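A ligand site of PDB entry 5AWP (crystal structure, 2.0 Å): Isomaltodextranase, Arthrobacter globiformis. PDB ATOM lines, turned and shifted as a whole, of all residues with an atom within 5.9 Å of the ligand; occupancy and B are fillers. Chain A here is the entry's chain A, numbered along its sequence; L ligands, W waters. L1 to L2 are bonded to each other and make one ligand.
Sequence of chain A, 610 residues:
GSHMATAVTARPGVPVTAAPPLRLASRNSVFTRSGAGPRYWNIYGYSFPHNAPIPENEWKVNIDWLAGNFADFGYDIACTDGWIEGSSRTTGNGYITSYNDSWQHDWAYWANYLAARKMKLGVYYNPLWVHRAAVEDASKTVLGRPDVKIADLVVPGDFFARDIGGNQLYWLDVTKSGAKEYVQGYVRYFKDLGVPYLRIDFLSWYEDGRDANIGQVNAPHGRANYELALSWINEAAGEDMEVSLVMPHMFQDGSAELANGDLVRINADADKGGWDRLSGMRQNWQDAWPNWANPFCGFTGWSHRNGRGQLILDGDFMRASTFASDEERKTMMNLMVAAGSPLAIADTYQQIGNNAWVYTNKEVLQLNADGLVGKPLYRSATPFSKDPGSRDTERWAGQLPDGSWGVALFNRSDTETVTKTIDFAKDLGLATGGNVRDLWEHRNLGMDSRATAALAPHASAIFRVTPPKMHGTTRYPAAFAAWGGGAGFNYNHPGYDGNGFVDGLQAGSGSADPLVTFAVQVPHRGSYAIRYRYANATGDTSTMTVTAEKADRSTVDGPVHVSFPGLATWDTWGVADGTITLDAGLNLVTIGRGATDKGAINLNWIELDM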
ATOM      1  N   TYR A  44       4.263  -2.340 -15.826  1.00  0.00           N
ATOM      2  CA  TYR A  44       3.525  -3.572 -16.116  1.00  0.00           C
ATOM      3  C   TYR A  44       3.845  -4.172 -17.486  1.00  0.00           C
ATOM      4  O   TYR A  44       3.846  -5.396 -17.625  1.00  0.00           O
ATOM      5  CB  TYR A  44       2.033  -3.291 -16.019  1.00  0.00           C
ATOM      6  CG  TYR A  44       1.107  -4.499 -16.028  1.00  0.00           C
ATOM      7  CD1 TYR A  44       0.853  -5.219 -14.859  1.00  0.00           C
ATOM      8  CD2 TYR A  44       0.447  -4.893 -17.186  1.00  0.00           C
ATOM      9  CE1 TYR A  44       0.009  -6.317 -14.853  1.00  0.00           C
ATOM     10  CE2 TYR A  44      -0.416  -5.974 -17.198  1.00  0.00           C
ATOM     11  CZ  TYR A  44      -0.653  -6.662 -16.034  1.00  0.00           C
ATOM     12  OH  TYR A  44      -1.523  -7.717 -16.028  1.00  0.00           O
ATOM     13  N   ASN A  51       6.917 -11.866 -16.280  1.00  0.00           N
ATOM     14  CA  ASN A  51       6.576 -12.358 -14.941  1.00  0.00           C
ATOM     15  C   ASN A  51       7.749 -12.161 -14.014  1.00  0.00           C
ATOM     16  O   ASN A  51       8.205 -13.081 -13.380  1.00  0.00           O
ATOM     17  CB  ASN A  51       6.133 -13.834 -14.979  1.00  0.00           C
ATOM     18  CG  ASN A  51       5.573 -14.327 -13.659  1.00  0.00           C
ATOM     19  OD1 ASN A  51       5.007 -13.558 -12.865  1.00  0.00           O
ATOM     20  ND2 ASN A  51       5.688 -15.624 -13.414  1.00  0.00           N
ATOM     21  N   ASP A  81       5.261  -1.261  -9.984  1.00  0.00           N
ATOM     22  CA  ASP A  81       4.132  -2.155  -9.847  1.00  0.00           C
ATOM     23  C   ASP A  81       4.516  -3.328  -8.925  1.00  0.00           C
ATOM     24  O   ASP A  81       5.304  -3.139  -7.976  1.00  0.00           O
ATOM     25  CB  ASP A  81       3.640  -2.601 -11.216  1.00  0.00           C
ATOM     26  CG  ASP A  81       2.177  -3.011 -11.203  1.00  0.00           C
ATOM     27  OD1 ASP A  81       1.314  -2.128 -11.085  1.00  0.00           O
ATOM     28  OD2 ASP A  81       1.897  -4.226 -11.242  1.00  0.00           O
ATOM     29  N   GLY A  82       3.951  -4.509  -9.173  1.00  0.00           N
ATOM     30  CA  GLY A  82       4.121  -5.652  -8.303  1.00  0.00           C
ATOM     31  C   GLY A  82       5.454  -6.326  -8.522  1.00  0.00           C
ATOM     32  O   GLY A  82       6.433  -5.681  -8.885  1.00  0.00           O
ATOM     33  N   TRP A  83       5.486  -7.630  -8.310  1.00  0.00           N
ATOM     34  CA  TRP A  83       6.723  -8.419  -8.280  1.00  0.00           C
ATOM     35  C   TRP A  83       7.657  -7.862  -7.212  1.00  0.00           C
ATOM     36  O   TRP A  83       8.839  -7.737  -7.438  1.00  0.00           O
ATOM     37  CB  TRP A  83       7.355  -8.525  -9.707  1.00  0.00           C
ATOM     38  CG  TRP A  83       6.420  -9.263 -10.650  1.00  0.00           C
ATOM     39  CD1 TRP A  83       6.388 -10.619 -10.910  1.00  0.00           C
ATOM     40  CD2 TRP A  83       5.318  -8.690 -11.392  1.00  0.00           C
ATOM     41  NE1 TRP A  83       5.359 -10.908 -11.777  1.00  0.00           N
ATOM     42  CE2 TRP A  83       4.693  -9.748 -12.091  1.00  0.00           C
ATOM     43  CE3 TRP A  83       4.818  -7.390 -11.554  1.00  0.00           C
ATOM     44  CZ2 TRP A  83       3.591  -9.548 -12.939  1.00  0.00           C
ATOM     45  CZ3 TRP A  83       3.706  -7.195 -12.383  1.00  0.00           C
ATOM     46  CH2 TRP A  83       3.096  -8.269 -13.051  1.00  0.00           C
ATOM     47  N   ILE A  84       7.096  -7.543  -6.031  1.00  0.00           N
ATOM     48  CA  ILE A  84       7.884  -6.920  -4.967  1.00  0.00           C
ATOM     49  C   ILE A  84       8.322  -7.876  -3.855  1.00  0.00           C
ATOM     50  O   ILE A  84       8.882  -7.424  -2.865  1.00  0.00           O
ATOM     51  CB  ILE A  84       7.228  -5.631  -4.372  1.00  0.00           C
ATOM     52  CG1 ILE A  84       5.745  -5.828  -4.060  1.00  0.00           C
ATOM     53  CG2 ILE A  84       7.424  -4.451  -5.321  1.00  0.00           C
ATOM     54  CD1 ILE A  84       5.498  -6.956  -3.076  1.00  0.00           C
ATOM     55  N   GLU A  85       8.104  -9.186  -4.027  1.00  0.00           N
ATOM     56  CA  GLU A  85       8.543 -10.144  -2.998  1.00  0.00           C
ATOM     57  C   GLU A  85      10.044 -10.086  -2.783  1.00  0.00           C
ATOM     58  O   GLU A  85      10.532 -10.295  -1.675  1.00  0.00           O
ATOM     59  CB  GLU A  85       8.128 -11.576  -3.367  1.00  0.00           C
ATOM     60  CG  GLU A  85       6.664 -11.912  -3.087  1.00  0.00           C
ATOM     61  CD  GLU A  85       5.657 -11.399  -4.129  1.00  0.00           C
ATOM     62  OE1 GLU A  85       6.042 -10.714  -5.095  1.00  0.00           O
ATOM     63  OE2 GLU A  85       4.452 -11.681  -3.941  1.00  0.00           O
ATOM     64  N   TYR A 124       3.902   1.340  -6.103  1.00  0.00           N
ATOM     65  CA  TYR A 124       2.979   0.246  -5.785  1.00  0.00           C
ATOM     66  C   TYR A 124       3.469  -0.410  -4.522  1.00  0.00           C
ATOM     67  O   TYR A 124       4.550  -1.012  -4.506  1.00  0.00           O
ATOM     68  CB  TYR A 124       2.990  -0.753  -6.924  1.00  0.00           C
ATOM     69  CG  TYR A 124       2.202  -2.035  -6.761  1.00  0.00           C
ATOM     70  CD1 TYR A 124       2.720  -3.076  -6.021  1.00  0.00           C
ATOM     71  CD2 TYR A 124       0.997  -2.251  -7.454  1.00  0.00           C
ATOM     72  CE1 TYR A 124       2.061  -4.273  -5.893  1.00  0.00           C
ATOM     73  CE2 TYR A 124       0.321  -3.473  -7.314  1.00  0.00           C
ATOM     74  CZ  TYR A 124       0.885  -4.476  -6.529  1.00  0.00           C
ATOM     75  OH  TYR A 124       0.328  -5.724  -6.338  1.00  0.00           O
ATOM     76  N   TRP A 129       1.741  -4.890   4.331  1.00  0.00           N
ATOM     77  CA  TRP A 129       2.714  -5.933   4.144  1.00  0.00           C
ATOM     78  C   TRP A 129       3.875  -5.670   5.089  1.00  0.00           C
ATOM     79  O   TRP A 129       4.310  -4.526   5.266  1.00  0.00           O
ATOM     80  CB  TRP A 129       3.258  -5.991   2.699  1.00  0.00           C
ATOM     81  CG  TRP A 129       2.357  -6.647   1.716  1.00  0.00           C
ATOM     82  CD1 TRP A 129       1.535  -7.701   1.932  1.00  0.00           C
ATOM     83  CD2 TRP A 129       2.217  -6.302   0.328  1.00  0.00           C
ATOM     84  NE1 TRP A 129       0.890  -8.046   0.766  1.00  0.00           N
ATOM     85  CE2 TRP A 129       1.285  -7.201  -0.236  1.00  0.00           C
ATOM     86  CE3 TRP A 129       2.768  -5.307  -0.489  1.00  0.00           C
ATOM     87  CZ2 TRP A 129       0.886  -7.147  -1.574  1.00  0.00           C
ATOM     88  CZ3 TRP A 129       2.375  -5.254  -1.840  1.00  0.00           C
ATOM     89  CH2 TRP A 129       1.440  -6.187  -2.356  1.00  0.00           C
ATOM     90  N   PHE A 160       0.873 -13.362   3.404  1.00  0.00           N
ATOM     91  CA  PHE A 160       0.190 -12.980   2.169  1.00  0.00           C
ATOM     92  C   PHE A 160       0.291 -14.139   1.191  1.00  0.00           C
ATOM     93  O   PHE A 160       1.377 -14.640   0.961  1.00  0.00           O
ATOM     94  CB  PHE A 160       0.874 -11.741   1.556  1.00  0.00           C
ATOM     95  CG  PHE A 160       0.527 -11.477   0.116  1.00  0.00           C
ATOM     96  CD1 PHE A 160      -0.772 -11.202  -0.245  1.00  0.00           C
ATOM     97  CD2 PHE A 160       1.511 -11.456  -0.868  1.00  0.00           C
ATOM     98  CE1 PHE A 160      -1.114 -10.942  -1.567  1.00  0.00           C
ATOM     99  CE2 PHE A 160       1.183 -11.187  -2.185  1.00  0.00           C
ATOM    100  CZ  PHE A 160      -0.133 -10.944  -2.542  1.00  0.00           C
ATOM    101  N   LEU A 169       6.080 -12.192   2.368  1.00  0.00           N
ATOM    102  CA  LEU A 169       5.369 -11.080   2.976  1.00  0.00           C
ATOM    103  C   LEU A 169       4.361 -11.574   3.985  1.00  0.00           C
ATOM    104  O   LEU A 169       3.547 -12.475   3.660  1.00  0.00           O
ATOM    105  CB  LEU A 169       4.654 -10.259   1.881  1.00  0.00           C
ATOM    106  CG  LEU A 169       5.541  -9.642   0.794  1.00  0.00           C
ATOM    107  CD1 LEU A 169       4.673  -9.160  -0.349  1.00  0.00           C
ATOM    108  CD2 LEU A 169       6.429  -8.503   1.316  1.00  0.00           C
ATOM    109  N   ARG A 199      -0.223   3.112  -4.988  1.00  0.00           N
ATOM    110  CA  ARG A 199      -1.097   2.143  -5.598  1.00  0.00           C
ATOM    111  C   ARG A 199      -1.109   0.917  -4.707  1.00  0.00           C
ATOM    112  O   ARG A 199      -0.091   0.189  -4.603  1.00  0.00           O
ATOM    113  CB  ARG A 199      -0.525   1.828  -6.981  1.00  0.00           C
ATOM    114  CG  ARG A 199      -1.432   1.018  -7.851  1.00  0.00           C
ATOM    115  CD  ARG A 199      -1.126   1.249  -9.337  1.00  0.00           C
ATOM    116  NE  ARG A 199      -2.005   0.406 -10.146  1.00  0.00           N
ATOM    117  CZ  ARG A 199      -3.234   0.729 -10.530  1.00  0.00           C
ATOM    118  NH1 ARG A 199      -3.795   1.888 -10.204  1.00  0.00           N
ATOM    119  NH2 ARG A 199      -3.922  -0.142 -11.260  1.00  0.00           N
ATOM    120  N   ASP A 201      -2.627  -2.574  -3.457  1.00  0.00           N
ATOM    121  CA  ASP A 201      -3.281  -3.745  -4.026  1.00  0.00           C
ATOM    122  C   ASP A 201      -3.398  -4.829  -2.963  1.00  0.00           C
ATOM    123  O   ASP A 201      -2.738  -4.767  -1.922  1.00  0.00           O
ATOM    124  CB  ASP A 201      -2.416  -4.230  -5.204  1.00  0.00           C
ATOM    125  CG  ASP A 201      -3.077  -5.307  -6.054  1.00  0.00           C
ATOM    126  OD1 ASP A 201      -4.305  -5.479  -5.964  1.00  0.00           O
ATOM    127  OD2 ASP A 201      -2.338  -5.952  -6.837  1.00  0.00           O
ATOM    128  N   PHE A 202      -4.216  -5.838  -3.263  1.00  0.00           N
ATOM    129  CA  PHE A 202      -4.371  -7.071  -2.460  1.00  0.00           C
ATOM    130  C   PHE A 202      -5.169  -6.897  -1.153  1.00  0.00           C
ATOM    131  O   PHE A 202      -5.168  -7.815  -0.305  1.00  0.00           O
ATOM    132  CB  PHE A 202      -3.036  -7.800  -2.266  1.00  0.00           C
ATOM    133  CG  PHE A 202      -2.528  -8.437  -3.534  1.00  0.00           C
ATOM    134  CD1 PHE A 202      -3.100  -9.621  -4.007  1.00  0.00           C
ATOM    135  CD2 PHE A 202      -1.515  -7.849  -4.268  1.00  0.00           C
ATOM    136  CE1 PHE A 202      -2.677 -10.196  -5.178  1.00  0.00           C
ATOM    137  CE2 PHE A 202      -1.083  -8.427  -5.465  1.00  0.00           C
ATOM    138  CZ  PHE A 202      -1.660  -9.602  -5.918  1.00  0.00           C
ATOM    139  N   VAL A 246      -6.404  -0.951  -5.541  1.00  0.00           N
ATOM    140  CA  VAL A 246      -6.289  -1.774  -6.748  1.00  0.00           C
ATOM    141  C   VAL A 246      -7.122  -3.070  -6.656  1.00  0.00           C
ATOM    142  O   VAL A 246      -7.455  -3.659  -7.686  1.00  0.00           O
ATOM    143  CB  VAL A 246      -4.812  -2.104  -7.022  1.00  0.00           C
ATOM    144  CG1 VAL A 246      -4.601  -2.951  -8.280  1.00  0.00           C
ATOM    145  CG2 VAL A 246      -4.013  -0.814  -7.150  1.00  0.00           C
ATOM    146  N   SME A 247      -7.468  -3.511  -5.439  1.00  0.00           N
ATOM    147  CA  SME A 247      -8.316  -4.720  -5.278  1.00  0.00           C
ATOM    148  CB  SME A 247      -7.478  -5.930  -4.920  1.00  0.00           C
ATOM    149  CG  SME A 247      -8.280  -7.186  -5.226  1.00  0.00           C
ATOM    150  S   SME A 247      -7.598  -8.598  -4.557  1.00  0.00           S
ATOM    151  OE  SME A 247      -7.124  -8.292  -3.188  1.00  0.00           O
ATOM    152  CE  SME A 247      -6.216  -8.846  -5.567  1.00  0.00           C
ATOM    153  C   SME A 247      -9.410  -4.509  -4.255  1.00  0.00           C
ATOM    154  O   SME A 247      -9.451  -5.167  -3.199  1.00  0.00           O
ATOM    155  N   ARG A 265     -10.039   0.439  -8.792  1.00  0.00           N
ATOM    156  CA  ARG A 265     -10.060  -0.392  -9.999  1.00  0.00           C
ATOM    157  C   ARG A 265     -11.471  -0.933 -10.212  1.00  0.00           C
ATOM    158  O   ARG A 265     -12.132  -1.376  -9.252  1.00  0.00           O
ATOM    159  CB  ARG A 265      -9.041  -1.554  -9.910  1.00  0.00           C
ATOM    160  CG  ARG A 265      -7.663  -1.197 -10.480  1.00  0.00           C
ATOM    161  CD  ARG A 265      -7.537  -1.491 -11.969  1.00  0.00           C
ATOM    162  NE  ARG A 265      -7.827  -2.914 -12.181  1.00  0.00           N
ATOM    163  CZ  ARG A 265      -6.979  -3.905 -11.903  1.00  0.00           C
ATOM    164  NH1 ARG A 265      -5.762  -3.634 -11.495  1.00  0.00           N
ATOM    165  NH2 ARG A 265      -7.350  -5.175 -12.011  1.00  0.00           N
ATOM    166  N   ASP A 269      -7.466  -7.272 -14.326  1.00  0.00           N
ATOM    167  CA  ASP A 269      -6.191  -6.759 -14.793  1.00  0.00           C
ATOM    168  C   ASP A 269      -6.121  -6.646 -16.309  1.00  0.00           C
ATOM    169  O   ASP A 269      -6.651  -7.497 -17.022  1.00  0.00           O
ATOM    170  CB  ASP A 269      -5.054  -7.737 -14.454  1.00  0.00           C
ATOM    171  CG  ASP A 269      -4.855  -7.950 -13.003  1.00  0.00           C
ATOM    172  OD1 ASP A 269      -5.592  -7.390 -12.133  1.00  0.00           O
ATOM    173  OD2 ASP A 269      -3.922  -8.729 -12.744  1.00  0.00           O
ATOM    174  N   TRP A 289     -14.559  -9.399  -5.845  1.00  0.00           N
ATOM    175  CA  TRP A 289     -13.560  -8.697  -6.666  1.00  0.00           C
ATOM    176  C   TRP A 289     -13.210  -9.498  -7.918  1.00  0.00           C
ATOM    177  O   TRP A 289     -12.949 -10.695  -7.810  1.00  0.00           O
ATOM    178  CB  TRP A 289     -12.259  -8.453  -5.891  1.00  0.00           C
ATOM    179  CG  TRP A 289     -11.121  -8.278  -6.838  1.00  0.00           C
ATOM    180  CD1 TRP A 289     -10.194  -9.225  -7.192  1.00  0.00           C
ATOM    181  CD2 TRP A 289     -10.831  -7.122  -7.624  1.00  0.00           C
ATOM    182  NE1 TRP A 289      -9.360  -8.727  -8.157  1.00  0.00           N
ATOM    183  CE2 TRP A 289      -9.703  -7.420  -8.417  1.00  0.00           C
ATOM    184  CE3 TRP A 289     -11.396  -5.851  -7.725  1.00  0.00           C
ATOM    185  CZ2 TRP A 289      -9.130  -6.508  -9.294  1.00  0.00           C
ATOM    186  CZ3 TRP A 289     -10.848  -4.927  -8.613  1.00  0.00           C
ATOM    187  CH2 TRP A 289      -9.712  -5.269  -9.391  1.00  0.00           C
ATOM    188  N   ASP A 316      -7.318   0.699 -15.145  1.00  0.00           N
ATOM    189  CA  ASP A 316      -6.037  -0.030 -15.149  1.00  0.00           C
ATOM    190  C   ASP A 316      -5.077   0.476 -16.225  1.00  0.00           C
ATOM    191  O   ASP A 316      -4.922   1.699 -16.376  1.00  0.00           O
ATOM    192  CB  ASP A 316      -6.219  -1.546 -15.170  1.00  0.00           C
ATOM    193  CG  ASP A 316      -5.009  -2.286 -14.604  1.00  0.00           C
ATOM    194  OD1 ASP A 316      -4.487  -1.900 -13.546  1.00  0.00           O
ATOM    195  OD2 ASP A 316      -4.576  -3.272 -15.230  1.00  0.00           O
ATOM    196  N   PHE A 317      -4.406  -0.414 -16.957  1.00  0.00           N
ATOM    197  CA  PHE A 317      -3.299  -0.024 -17.793  1.00  0.00           C
ATOM    198  C   PHE A 317      -3.609  -0.124 -19.278  1.00  0.00           C
ATOM    199  O   PHE A 317      -4.251  -1.046 -19.715  1.00  0.00           O
ATOM    200  CB  PHE A 317      -2.103  -0.908 -17.508  1.00  0.00           C
ATOM    201  CG  PHE A 317      -1.663  -0.893 -16.084  1.00  0.00           C
ATOM    202  CD1 PHE A 317      -1.605   0.284 -15.358  1.00  0.00           C
ATOM    203  CD2 PHE A 317      -1.222  -2.068 -15.476  1.00  0.00           C
ATOM    204  CE1 PHE A 317      -1.190   0.295 -14.042  1.00  0.00           C
ATOM    205  CE2 PHE A 317      -0.771  -2.051 -14.154  1.00  0.00           C
ATOM    206  CZ  PHE A 317      -0.741  -0.859 -13.456  1.00  0.00           C
HETATM  207  C1  LIG L   1      -3.229  -6.290  -9.857  1.00  0.00           C
HETATM  208  C2  LIG L   1      -2.370  -5.878 -11.048  1.00  0.00           C
HETATM  209  C3  LIG L   1      -0.900  -6.060 -10.674  1.00  0.00           C
HETATM  210  C4  LIG L   1      -0.625  -7.488 -10.259  1.00  0.00           C
HETATM  211  C5  LIG L   1       0.809  -7.638  -9.773  1.00  0.00           C
HETATM  212  C6  LIG L   1      -2.896  -7.735  -9.456  1.00  0.00           C
HETATM  213  O1  LIG L   1      -3.609  -8.041  -8.263  1.00  0.00           O
HETATM  214  O2  LIG L   1      -4.639  -6.166 -10.132  1.00  0.00           O
HETATM  215  O3  LIG L   1      -2.602  -4.500 -11.371  1.00  0.00           O
HETATM  216  O4  LIG L   1      -0.046  -5.723 -11.775  1.00  0.00           O
HETATM  217  O5  LIG L   1      -1.497  -7.845  -9.194  1.00  0.00           O
HETATM  218  O6  LIG L   1       0.962  -9.002  -9.391  1.00  0.00           O
HETATM  219  C1  LG2 L   2       2.355  -9.301  -9.265  1.00  0.00           C
HETATM  220  C2  LG2 L   2       2.530 -10.828  -9.317  1.00  0.00           C
HETATM  221  C3  LG2 L   2       2.048 -11.521  -8.067  1.00  0.00           C
HETATM  222  C4  LG2 L   2       2.727 -10.849  -6.892  1.00  0.00           C
HETATM  223  C5  LG2 L   2       2.367  -9.360  -6.895  1.00  0.00           C
HETATM  224  C6  LG2 L   2       2.993  -8.593  -5.743  1.00  0.00           C
HETATM  225  O1  LG2 L   2       1.847 -11.378 -10.431  1.00  0.00           O
HETATM  226  O2  LG2 L   2       2.445 -12.868  -8.125  1.00  0.00           O
HETATM  227  O3  LG2 L   2       2.428 -11.483  -5.666  1.00  0.00           O
HETATM  228  O4  LG2 L   2       2.926  -8.784  -8.071  1.00  0.00           O
HETATM  229  O5  LG2 L   2       4.401  -8.715  -5.699  1.00  0.00           O
HETATM  230  O   HOH W   1      -1.037 -10.753  -9.621  1.00  0.00           O
HETATM  231  O   HOH W   2       2.773 -13.748 -11.393  1.00  0.00           O
HETATM  232  O   HOH W   3      -4.481 -10.518  -8.338  1.00  0.00           O
HETATM  233  O   HOH W   4      -6.551  -8.804  -9.407  1.00  0.00           O
HETATM  234  O   HOH W   5      -1.302  -2.399 -10.287  1.00  0.00           O
HETATM  235  O   HOH W   6      -6.065  -6.147  -7.974  1.00  0.00           O
HETATM  236  O   HOH W   7       5.265 -13.844  -8.319  1.00  0.00           O
HETATM  237  O   HOH W   8      -2.828  -4.951 -13.942  1.00  0.00           O
HETATM  238  O   HOH W   9       0.336 -10.687 -12.790  1.00  0.00           O
HETATM  239  O   HOH W  10       0.431 -13.283  -5.263  1.00  0.00           O
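The backbone NH of Ile 84 lies within hydrogen-bond range of an oxygen (O5) of LG2 L2, 3.0 Å away.
The side-chain carboxylate (OE1) of Glu 85 is in hydrogen-bond range of an oxygen (O5) of LG2 L2 (2.7 Å).
The side-chain carboxylate (OD2) of Asp 81 is in hydrogen-bond range of an oxygen (O4) of LIG L1 (2.5 Å).
The side-chain carboxylate of Asp 201 is in hydrogen-bond range of an oxygen (O1) of LIG L1 (2.8 Å).
OD1 of Asp 269 sits at hydrogen-bond distance from O2 of LIG L1.
O2 of LIG L1 is in hydrogen-bond range of NH1 of Arg 265 (3.1 Å).
O4 of LG2 L2 lies within hydrogen-bond range of N of Trp 83 (2.8 Å).
Water W6 lies within hydrogen-bond range of an oxygen (O2) of LIG L1, the side-chain carboxylate (OD1) of Asp 201 and the backbone carbonyl oxygen (O) of Val 246.
Water W8 bridges an oxygen (O3) of LIG L1 (2.6 Å) and the side-chain carboxylate (OD2) of Asp 316 (2.7 Å).
Water W5 lies within hydrogen-bond range of O3 of LIG L1 (2.7 Å), OD1 of Asp 81 (2.7 Å) and NE of Arg 199 (2.9 Å).
Water W2 lies within hydrogen-bond range of the side-chain amide oxygen (OD1) of Asn 51 (2.7 Å) and an oxygen (O1) of LG2 L2 (2.7 Å).
Water W4 lies within hydrogen-bond range of NE1 of Trp 289 (3.1 Å), OD1 of Asp 269 (3.2 Å) and O1 of LIG L1 (3.2 Å).
OD1 of Asp 316 lies within salt-bridge range of NH2 of Arg 199 (2.9 Å).
The side-chain amide oxygen of Asn 51 lies within hydrogen-bond range of the indole nitrogen of Trp 83 (2.9 Å).
The side-chain carboxylate of Asp 201 sits at hydrogen-bond distance from the side-chain hydroxyl of Tyr 124, 2.7 Å away.
OD1 of Asp 316 is in salt-bridge range of NH1 of Arg 265.
NH2 of Arg 265 lies within salt-bridge range of OD1 of Asp 269.
The backbone carbonyl oxygen of Leu 169 is in hydrogen-bond range of the backbone NH of Phe 160, 2.8 Å away.
CE1 of Tyr 44 touches O4 of LIG L1 (3.1 Å).
Gly 82 touches the ligand.
Tyr 124 touches the ligand.
Phe 160 touches the ligand.
CZ of Phe 202 touches O1 of LIG L1, at 3.4 Å.
CG1 of Val 246 touches O2 of LIG L1, at 3.7 Å.
SME 247 touches the ligand.
OD1 of Asp 316 touches O3 of LIG L1, 3.9 Å away.
Hydrophobic or aromatic side chains within 4 Å of the ligand: Tyr 44, Trp 83, Ile 84, Phe 160, Phe 202 and Val 246.
Of the 21 residues printed, 15 come within 4 Å of the ligand.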
